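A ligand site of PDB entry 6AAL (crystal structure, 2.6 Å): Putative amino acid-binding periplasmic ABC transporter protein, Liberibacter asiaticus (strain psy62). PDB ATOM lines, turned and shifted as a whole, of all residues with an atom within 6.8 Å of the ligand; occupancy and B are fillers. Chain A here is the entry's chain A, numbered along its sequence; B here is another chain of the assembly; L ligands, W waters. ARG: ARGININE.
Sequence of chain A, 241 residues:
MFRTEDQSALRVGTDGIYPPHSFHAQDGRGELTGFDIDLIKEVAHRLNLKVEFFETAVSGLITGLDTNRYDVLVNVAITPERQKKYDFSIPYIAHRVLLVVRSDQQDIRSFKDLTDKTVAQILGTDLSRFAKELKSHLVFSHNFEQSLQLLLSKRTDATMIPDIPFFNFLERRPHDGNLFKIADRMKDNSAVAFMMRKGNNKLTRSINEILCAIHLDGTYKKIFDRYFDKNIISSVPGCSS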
ATOM      1  N   VAL A  58     -23.459  30.858  -2.909  1.00  0.00           N
ATOM      2  CA  VAL A  58     -22.880  30.680  -1.603  1.00  0.00           C
ATOM      3  C   VAL A  58     -21.773  31.679  -1.318  1.00  0.00           C
ATOM      4  O   VAL A  58     -21.637  32.138  -0.206  1.00  0.00           O
ATOM      5  CB  VAL A  58     -22.394  29.223  -1.433  1.00  0.00           C
ATOM      6  CG1 VAL A  58     -21.292  29.108  -0.369  1.00  0.00           C
ATOM      7  CG2 VAL A  58     -23.570  28.303  -1.111  1.00  0.00           C
ATOM      8  N   ILE A  62     -23.128  35.092   3.266  1.00  0.00           N
ATOM      9  CA  ILE A  62     -22.888  35.765   4.559  1.00  0.00           C
ATOM     10  C   ILE A  62     -22.778  37.295   4.370  1.00  0.00           C
ATOM     11  O   ILE A  62     -23.356  38.042   5.137  1.00  0.00           O
ATOM     12  CB  ILE A  62     -21.650  35.192   5.295  1.00  0.00           C
ATOM     13  CG1 ILE A  62     -21.762  33.671   5.377  1.00  0.00           C
ATOM     14  CG2 ILE A  62     -21.491  35.802   6.691  1.00  0.00           C
ATOM     15  CD1 ILE A  62     -20.985  32.996   6.505  1.00  0.00           C
ATOM     16  N   ASN A  75     -29.154  26.713   6.913  1.00  0.00           N
ATOM     17  CA  ASN A  75     -28.112  25.686   6.826  1.00  0.00           C
ATOM     18  C   ASN A  75     -26.666  26.174   7.147  1.00  0.00           C
ATOM     19  O   ASN A  75     -25.717  25.780   6.441  1.00  0.00           O
ATOM     20  CB  ASN A  75     -28.172  25.023   5.431  1.00  0.00           C
ATOM     21  CG  ASN A  75     -27.292  23.785   5.313  1.00  0.00           C
ATOM     22  OD1 ASN A  75     -26.890  23.215   6.317  1.00  0.00           O
ATOM     23  ND2 ASN A  75     -26.975  23.387   4.081  1.00  0.00           N
ATOM     24  N   VAL A  76     -26.506  27.011   8.189  1.00  0.00           N
ATOM     25  CA  VAL A  76     -25.175  27.514   8.607  1.00  0.00           C
ATOM     26  C   VAL A  76     -24.550  26.727   9.750  1.00  0.00           C
ATOM     27  O   VAL A  76     -25.067  26.700  10.851  1.00  0.00           O
ATOM     28  CB  VAL A  76     -25.212  28.952   9.105  1.00  0.00           C
ATOM     29  CG1 VAL A  76     -23.787  29.528   9.168  1.00  0.00           C
ATOM     30  CG2 VAL A  76     -26.089  29.802   8.215  1.00  0.00           C
ATOM     31  N   ALA A  77     -23.400  26.121   9.511  1.00  0.00           N
ATOM     32  CA  ALA A  77     -22.689  25.448  10.560  1.00  0.00           C
ATOM     33  C   ALA A  77     -22.148  26.477  11.543  1.00  0.00           C
ATOM     34  O   ALA A  77     -21.418  27.391  11.154  1.00  0.00           O
ATOM     35  CB  ALA A  77     -21.555  24.595   9.976  1.00  0.00           C
ATOM     36  N   ILE A  78     -22.467  26.290  12.812  1.00  0.00           N
ATOM     37  CA  ILE A  78     -22.023  27.164  13.892  1.00  0.00           C
ATOM     38  C   ILE A  78     -20.542  27.059  14.102  1.00  0.00           C
ATOM     39  O   ILE A  78     -20.028  25.998  14.377  1.00  0.00           O
ATOM     40  CB  ILE A  78     -22.700  26.777  15.217  1.00  0.00           C
ATOM     41  CG1 ILE A  78     -24.242  26.961  15.100  1.00  0.00           C
ATOM     42  CG2 ILE A  78     -22.095  27.557  16.362  1.00  0.00           C
ATOM     43  CD1 ILE A  78     -25.029  26.632  16.344  1.00  0.00           C
ATOM     44  N   THR A  79     -19.851  28.173  13.956  1.00  0.00           N
ATOM     45  CA  THR A  79     -18.450  28.260  14.348  1.00  0.00           C
ATOM     46  C   THR A  79     -18.266  29.361  15.383  1.00  0.00           C
ATOM     47  O   THR A  79     -19.068  30.305  15.469  1.00  0.00           O
ATOM     48  CB  THR A  79     -17.540  28.691  13.193  1.00  0.00           C
ATOM     49  OG1 THR A  79     -17.990  29.982  12.730  1.00  0.00           O
ATOM     50  CG2 THR A  79     -17.535  27.692  12.048  1.00  0.00           C
ATOM     51  N   ARG A  82     -18.211  32.851  13.798  1.00  0.00           N
ATOM     52  CA  ARG A  82     -19.536  33.331  13.429  1.00  0.00           C
ATOM     53  C   ARG A  82     -20.388  33.573  14.642  1.00  0.00           C
ATOM     54  O   ARG A  82     -21.313  34.378  14.590  1.00  0.00           O
ATOM     55  CB  ARG A  82     -20.255  32.355  12.511  1.00  0.00           C
ATOM     56  CG  ARG A  82     -19.659  32.239  11.114  1.00  0.00           C
ATOM     57  CD  ARG A  82     -20.180  30.998  10.430  1.00  0.00           C
ATOM     58  NE  ARG A  82     -19.513  30.666   9.178  1.00  0.00           N
ATOM     59  CZ  ARG A  82     -19.798  29.585   8.451  1.00  0.00           C
ATOM     60  NH1 ARG A  82     -20.744  28.737   8.838  1.00  0.00           N
ATOM     61  NH2 ARG A  82     -19.146  29.352   7.334  1.00  0.00           N
ATOM     62  N   HIS A  95     -24.727  17.989  10.969  1.00  0.00           N
ATOM     63  CA  HIS A  95     -24.086  17.249   9.904  1.00  0.00           C
ATOM     64  C   HIS A  95     -22.705  16.744  10.271  1.00  0.00           C
ATOM     65  O   HIS A  95     -22.137  17.117  11.305  1.00  0.00           O
ATOM     66  CB  HIS A  95     -24.136  18.010   8.560  1.00  0.00           C
ATOM     67  CG  HIS A  95     -23.248  19.203   8.478  1.00  0.00           C
ATOM     68  ND1 HIS A  95     -23.641  20.360   7.828  1.00  0.00           N
ATOM     69  CD2 HIS A  95     -21.980  19.420   8.896  1.00  0.00           C
ATOM     70  CE1 HIS A  95     -22.646  21.241   7.863  1.00  0.00           C
ATOM     71  NE2 HIS A  95     -21.629  20.690   8.504  1.00  0.00           N
ATOM     72  N   ARG A  96     -22.180  15.870   9.405  1.00  0.00           N
ATOM     73  CA  ARG A  96     -20.923  15.162   9.671  1.00  0.00           C
ATOM     74  C   ARG A  96     -20.020  15.385   8.471  1.00  0.00           C
ATOM     75  O   ARG A  96     -20.406  15.071   7.351  1.00  0.00           O
ATOM     76  CB  ARG A  96     -21.191  13.673   9.846  1.00  0.00           C
ATOM     77  CG  ARG A  96     -20.032  12.924  10.447  1.00  0.00           C
ATOM     78  CD  ARG A  96     -20.046  13.133  11.939  1.00  0.00           C
ATOM     79  NE  ARG A  96     -18.875  12.581  12.597  1.00  0.00           N
ATOM     80  CZ  ARG A  96     -18.729  11.302  12.901  1.00  0.00           C
ATOM     81  NH1 ARG A  96     -19.676  10.416  12.582  1.00  0.00           N
ATOM     82  NH2 ARG A  96     -17.619  10.911  13.508  1.00  0.00           N
ATOM     83  N   VAL A  97     -18.839  15.910   8.725  1.00  0.00           N
ATOM     84  CA  VAL A  97     -17.940  16.334   7.652  1.00  0.00           C
ATOM     85  C   VAL A  97     -17.070  15.137   7.254  1.00  0.00           C
ATOM     86  O   VAL A  97     -16.263  14.621   8.044  1.00  0.00           O
ATOM     87  CB  VAL A  97     -17.136  17.596   8.050  1.00  0.00           C
ATOM     88  CG1 VAL A  97     -15.971  17.849   7.085  1.00  0.00           C
ATOM     89  CG2 VAL A  97     -18.049  18.820   8.035  1.00  0.00           C
ATOM     90  N   GLY A 124     -15.636  30.373  -1.318  1.00  0.00           N
ATOM     91  CA  GLY A 124     -16.101  31.149  -0.158  1.00  0.00           C
ATOM     92  C   GLY A 124     -16.593  30.390   1.060  1.00  0.00           C
ATOM     93  O   GLY A 124     -17.172  30.997   1.953  1.00  0.00           O
ATOM     94  N   THR A 125     -16.374  29.063   1.129  1.00  0.00           N
ATOM     95  CA  THR A 125     -16.837  28.262   2.279  1.00  0.00           C
ATOM     96  C   THR A 125     -15.688  28.087   3.258  1.00  0.00           C
ATOM     97  O   THR A 125     -14.542  28.441   2.931  1.00  0.00           O
ATOM     98  CB  THR A 125     -17.369  26.880   1.856  1.00  0.00           C
ATOM     99  OG1 THR A 125     -16.367  26.214   1.068  1.00  0.00           O
ATOM    100  CG2 THR A 125     -18.646  27.001   1.070  1.00  0.00           C
ATOM    101  N   ASP A 126     -15.976  27.575   4.452  1.00  0.00           N
ATOM    102  CA  ASP A 126     -14.937  27.280   5.451  1.00  0.00           C
ATOM    103  C   ASP A 126     -14.176  25.994   5.066  1.00  0.00           C
ATOM    104  O   ASP A 126     -12.955  25.916   5.221  1.00  0.00           O
ATOM    105  CB  ASP A 126     -15.537  27.144   6.853  1.00  0.00           C
ATOM    106  CG  ASP A 126     -15.752  28.484   7.541  1.00  0.00           C
ATOM    107  OD1 ASP A 126     -16.322  28.522   8.660  1.00  0.00           O
ATOM    108  OD2 ASP A 126     -15.354  29.510   6.971  1.00  0.00           O
ATOM    109  N   LEU A 127     -14.887  25.000   4.538  1.00  0.00           N
ATOM    110  CA  LEU A 127     -14.206  23.817   4.046  1.00  0.00           C
ATOM    111  C   LEU A 127     -13.219  24.166   2.978  1.00  0.00           C
ATOM    112  O   LEU A 127     -12.243  23.471   2.834  1.00  0.00           O
ATOM    113  CB  LEU A 127     -15.178  22.788   3.477  1.00  0.00           C
ATOM    114  CG  LEU A 127     -16.135  22.078   4.423  1.00  0.00           C
ATOM    115  CD1 LEU A 127     -16.927  21.069   3.613  1.00  0.00           C
ATOM    116  CD2 LEU A 127     -15.419  21.408   5.571  1.00  0.00           C
ATOM    117  N   SER A 128     -13.476  25.232   2.211  1.00  0.00           N
ATOM    118  CA  SER A 128     -12.531  25.667   1.157  1.00  0.00           C
ATOM    119  C   SER A 128     -11.301  26.383   1.730  1.00  0.00           C
ATOM    120  O   SER A 128     -10.180  26.245   1.246  1.00  0.00           O
ATOM    121  CB  SER A 128     -13.268  26.585   0.177  1.00  0.00           C
ATOM    122  OG  SER A 128     -12.385  27.413  -0.538  1.00  0.00           O
ATOM    123  N   ARG A 129     -11.538  27.172   2.774  1.00  0.00           N
ATOM    124  CA  ARG A 129     -10.469  27.738   3.581  1.00  0.00           C
ATOM    125  C   ARG A 129      -9.599  26.613   4.107  1.00  0.00           C
ATOM    126  O   ARG A 129      -8.372  26.692   4.042  1.00  0.00           O
ATOM    127  CB  ARG A 129     -11.076  28.504   4.749  1.00  0.00           C
ATOM    128  CG  ARG A 129     -10.136  29.480   5.461  1.00  0.00           C
ATOM    129  CD  ARG A 129     -10.944  30.510   6.265  1.00  0.00           C
ATOM    130  NE  ARG A 129     -12.032  31.069   5.447  1.00  0.00           N
ATOM    131  CZ  ARG A 129     -13.172  31.579   5.917  1.00  0.00           C
ATOM    132  NH1 ARG A 129     -13.412  31.644   7.232  1.00  0.00           N
ATOM    133  NH2 ARG A 129     -14.085  32.033   5.048  1.00  0.00           N
ATOM    134  N   PHE A 144     -22.081  21.009  -4.335  1.00  0.00           N
ATOM    135  CA  PHE A 144     -21.630  19.674  -3.951  1.00  0.00           C
ATOM    136  C   PHE A 144     -21.781  18.695  -5.112  1.00  0.00           C
ATOM    137  O   PHE A 144     -21.018  17.752  -5.234  1.00  0.00           O
ATOM    138  CB  PHE A 144     -22.407  19.148  -2.744  1.00  0.00           C
ATOM    139  CG  PHE A 144     -22.283  19.978  -1.501  1.00  0.00           C
ATOM    140  CD1 PHE A 144     -23.397  20.530  -0.908  1.00  0.00           C
ATOM    141  CD2 PHE A 144     -21.058  20.157  -0.888  1.00  0.00           C
ATOM    142  CE1 PHE A 144     -23.290  21.283   0.277  1.00  0.00           C
ATOM    143  CE2 PHE A 144     -20.924  20.892   0.285  1.00  0.00           C
ATOM    144  CZ  PHE A 144     -22.036  21.465   0.870  1.00  0.00           C
ATOM    145  N   PRO A 162     -20.168  17.447   3.633  1.00  0.00           N
ATOM    146  CA  PRO A 162     -20.950  16.887   4.749  1.00  0.00           C
ATOM    147  C   PRO A 162     -21.810  15.706   4.294  1.00  0.00           C
ATOM    148  O   PRO A 162     -22.030  15.530   3.091  1.00  0.00           O
ATOM    149  CB  PRO A 162     -21.813  18.047   5.243  1.00  0.00           C
ATOM    150  CG  PRO A 162     -21.349  19.269   4.513  1.00  0.00           C
ATOM    151  CD  PRO A 162     -20.438  18.874   3.383  1.00  0.00           C
ATOM    152  N   MET A 186     -14.603  13.921  10.320  1.00  0.00           N
ATOM    153  CA  MET A 186     -14.381  14.679  11.540  1.00  0.00           C
ATOM    154  C   MET A 186     -14.946  13.831  12.679  1.00  0.00           C
ATOM    155  O   MET A 186     -16.017  13.235  12.536  1.00  0.00           O
ATOM    156  CB  MET A 186     -15.017  16.079  11.457  1.00  0.00           C
ATOM    157  CG  MET A 186     -14.276  16.968  10.467  1.00  0.00           C
ATOM    158  SD  MET A 186     -12.607  17.158  11.071  1.00  0.00           S
ATOM    159  CE  MET A 186     -11.717  17.769   9.647  1.00  0.00           C
ATOM    160  N   ASN A 189     -19.790  15.380  14.919  1.00  0.00           N
ATOM    161  CA  ASN A 189     -20.715  16.007  14.009  1.00  0.00           C
ATOM    162  C   ASN A 189     -20.801  17.439  14.412  1.00  0.00           C
ATOM    163  O   ASN A 189     -20.249  17.832  15.432  1.00  0.00           O
ATOM    164  CB  ASN A 189     -22.081  15.358  14.047  1.00  0.00           C
ATOM    165  CG  ASN A 189     -22.727  15.414  15.386  1.00  0.00           C
ATOM    166  OD1 ASN A 189     -22.473  16.326  16.181  1.00  0.00           O
ATOM    167  ND2 ASN A 189     -23.550  14.421  15.665  1.00  0.00           N
ATOM    168  N   SER A 190     -21.481  18.227  13.603  1.00  0.00           N
ATOM    169  CA  SER A 190     -21.455  19.687  13.718  1.00  0.00           C
ATOM    170  C   SER A 190     -22.843  20.223  13.611  1.00  0.00           C
ATOM    171  O   SER A 190     -23.572  19.828  12.715  1.00  0.00           O
ATOM    172  CB  SER A 190     -20.618  20.281  12.595  1.00  0.00           C
ATOM    173  OG  SER A 190     -19.263  19.918  12.794  1.00  0.00           O
ATOM    174  N   ALA A 191     -23.200  21.103  14.542  1.00  0.00           N
ATOM    175  CA  ALA A 191     -24.497  21.735  14.576  1.00  0.00           C
ATOM    176  C   ALA A 191     -24.654  22.772  13.478  1.00  0.00           C
ATOM    177  O   ALA A 191     -23.694  23.471  13.071  1.00  0.00           O
ATOM    178  CB  ALA A 191     -24.770  22.400  15.917  1.00  0.00           C
ATOM    179  N   VAL A 192     -25.901  22.812  13.008  1.00  0.00           N
ATOM    180  CA  VAL A 192     -26.340  23.713  11.981  1.00  0.00           C
ATOM    181  C   VAL A 192     -27.557  24.484  12.513  1.00  0.00           C
ATOM    182  O   VAL A 192     -28.342  23.938  13.305  1.00  0.00           O
ATOM    183  CB  VAL A 192     -26.668  22.899  10.736  1.00  0.00           C
ATOM    184  CG1 VAL A 192     -27.296  23.780   9.676  1.00  0.00           C
ATOM    185  CG2 VAL A 192     -25.397  22.170  10.229  1.00  0.00           C
ATOM    186  N   CYS B 239     -19.438  21.136  17.032  1.00  0.00           N
ATOM    187  CA  CYS B 239     -19.350  22.474  16.426  1.00  0.00           C
ATOM    188  C   CYS B 239     -18.367  22.407  15.272  1.00  0.00           C
ATOM    189  O   CYS B 239     -17.893  21.321  14.914  1.00  0.00           O
ATOM    190  CB  CYS B 239     -18.840  23.436  17.467  1.00  0.00           C
ATOM    191  SG  CYS B 239     -19.855  24.879  17.661  1.00  0.00           S
ATOM    192  N   SER B 240     -18.052  23.559  14.682  1.00  0.00           N
ATOM    193  CA  SER B 240     -17.064  23.619  13.584  1.00  0.00           C
ATOM    194  C   SER B 240     -16.040  24.735  13.848  1.00  0.00           C
ATOM    195  O   SER B 240     -16.355  25.730  14.495  1.00  0.00           O
ATOM    196  CB  SER B 240     -17.776  23.832  12.230  1.00  0.00           C
ATOM    197  OG  SER B 240     -18.899  22.990  12.106  1.00  0.00           O
ATOM    198  N   SER B 241     -14.824  24.577  13.314  1.00  0.00           N
ATOM    199  CA  SER B 241     -13.742  25.536  13.584  1.00  0.00           C
ATOM    200  C   SER B 241     -14.027  26.916  13.021  1.00  0.00           C
ATOM    201  O   SER B 241     -14.368  27.030  11.854  1.00  0.00           O
ATOM    202  CB  SER B 241     -12.429  25.047  13.000  1.00  0.00           C
ATOM    203  OG  SER B 241     -12.457  23.649  12.857  1.00  0.00           O
HETATM  204  N   ARG L   1     -21.480  26.330   4.739  1.00  0.00           N
HETATM  205  CA  ARG L   1     -20.459  26.439   5.826  1.00  0.00           C
HETATM  206  C   ARG L   1     -19.134  26.438   5.188  1.00  0.00           C
HETATM  207  O   ARG L   1     -18.650  27.493   4.837  1.00  0.00           O
HETATM  208  CB  ARG L   1     -20.591  25.328   6.847  1.00  0.00           C
HETATM  209  CG  ARG L   1     -20.425  23.904   6.293  1.00  0.00           C
HETATM  210  CD  ARG L   1     -19.122  23.254   6.765  1.00  0.00           C
HETATM  211  NE  ARG L   1     -19.344  22.541   8.029  1.00  0.00           N
HETATM  212  CZ  ARG L   1     -18.420  22.314   8.958  1.00  0.00           C
HETATM  213  NH1 ARG L   1     -18.768  21.645  10.048  1.00  0.00           N
HETATM  214  NH2 ARG L   1     -17.179  22.772   8.819  1.00  0.00           N
HETATM  215  OXT ARG L   1     -18.474  25.444   4.977  1.00  0.00           O
HETATM  216  O   HOH W   1     -22.286  25.385   1.851  1.00  0.00           O
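Residues that only touch the ligand: Thr 125 (3.2 Å), Ala 77 (3.4 Å), Val 97 (3.5 Å) and Leu 127 (3.6 Å). Hydrophobic or aromatic side chains that line the ligand: Ala 77, His 95, Val 97 and Leu 127. Within 4 Å of the ligand: Ala 77, Arg 82, His 95, Val 97, Thr 125, Asp 126, Leu 127, Ser 190 and Ser 240 of chain B. The nearest printed residue that does not touch the ligand is Asn 75 (4.6 Å).
The side-chain hydroxyl (OG) of Ser 240 of chain B sits at hydrogen-bond distance from a nitrogen (NH1) of the ligand (2.5 Å). N of Asp 126 lies within hydrogen-bond range of O of the ligand. A nitrogen (NE) of the ligand lies within hydrogen-bond range of a ring nitrogen (NE2) of His 95 (3.0 Å). The guanidinium group (NH2) of Arg 82 is in salt-bridge range of an oxygen (O) of the ligand (3.2 Å). The side-chain hydroxyl (OG) of Ser 190 is in hydrogen-bond range of a nitrogen (NH1) of the ligand (3.3 Å).
OG of Ser 240 of chain B lies within hydrogen-bond range of OG of Ser 190 (3.2 Å). The guanidinium group of Arg 82 lies within salt-bridge range of the side-chain carboxylate of Asp 126 (3.2 Å). OD2 of Asp 126 lies within salt-bridge range of NH1 of Arg 129, at 2.9 Å. O of His 95 lies within hydrogen-bond range of N of Ser 190 (2.6 Å). NH1 of Arg 82 lies within hydrogen-bond range of O of Ala 77 (2.8 Å). OG1 of Thr 79 sits at hydrogen-bond distance from N of Arg 82, at 3.1 Å. OG1 of Thr 125 sits close to N of Ser 128, 3.3 Å away. The side-chain hydroxyl (OG) of Ser 190 lies within hydrogen-bond range of the backbone carbonyl oxygen (O) of Cys 239 of chain B (2.9 Å).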
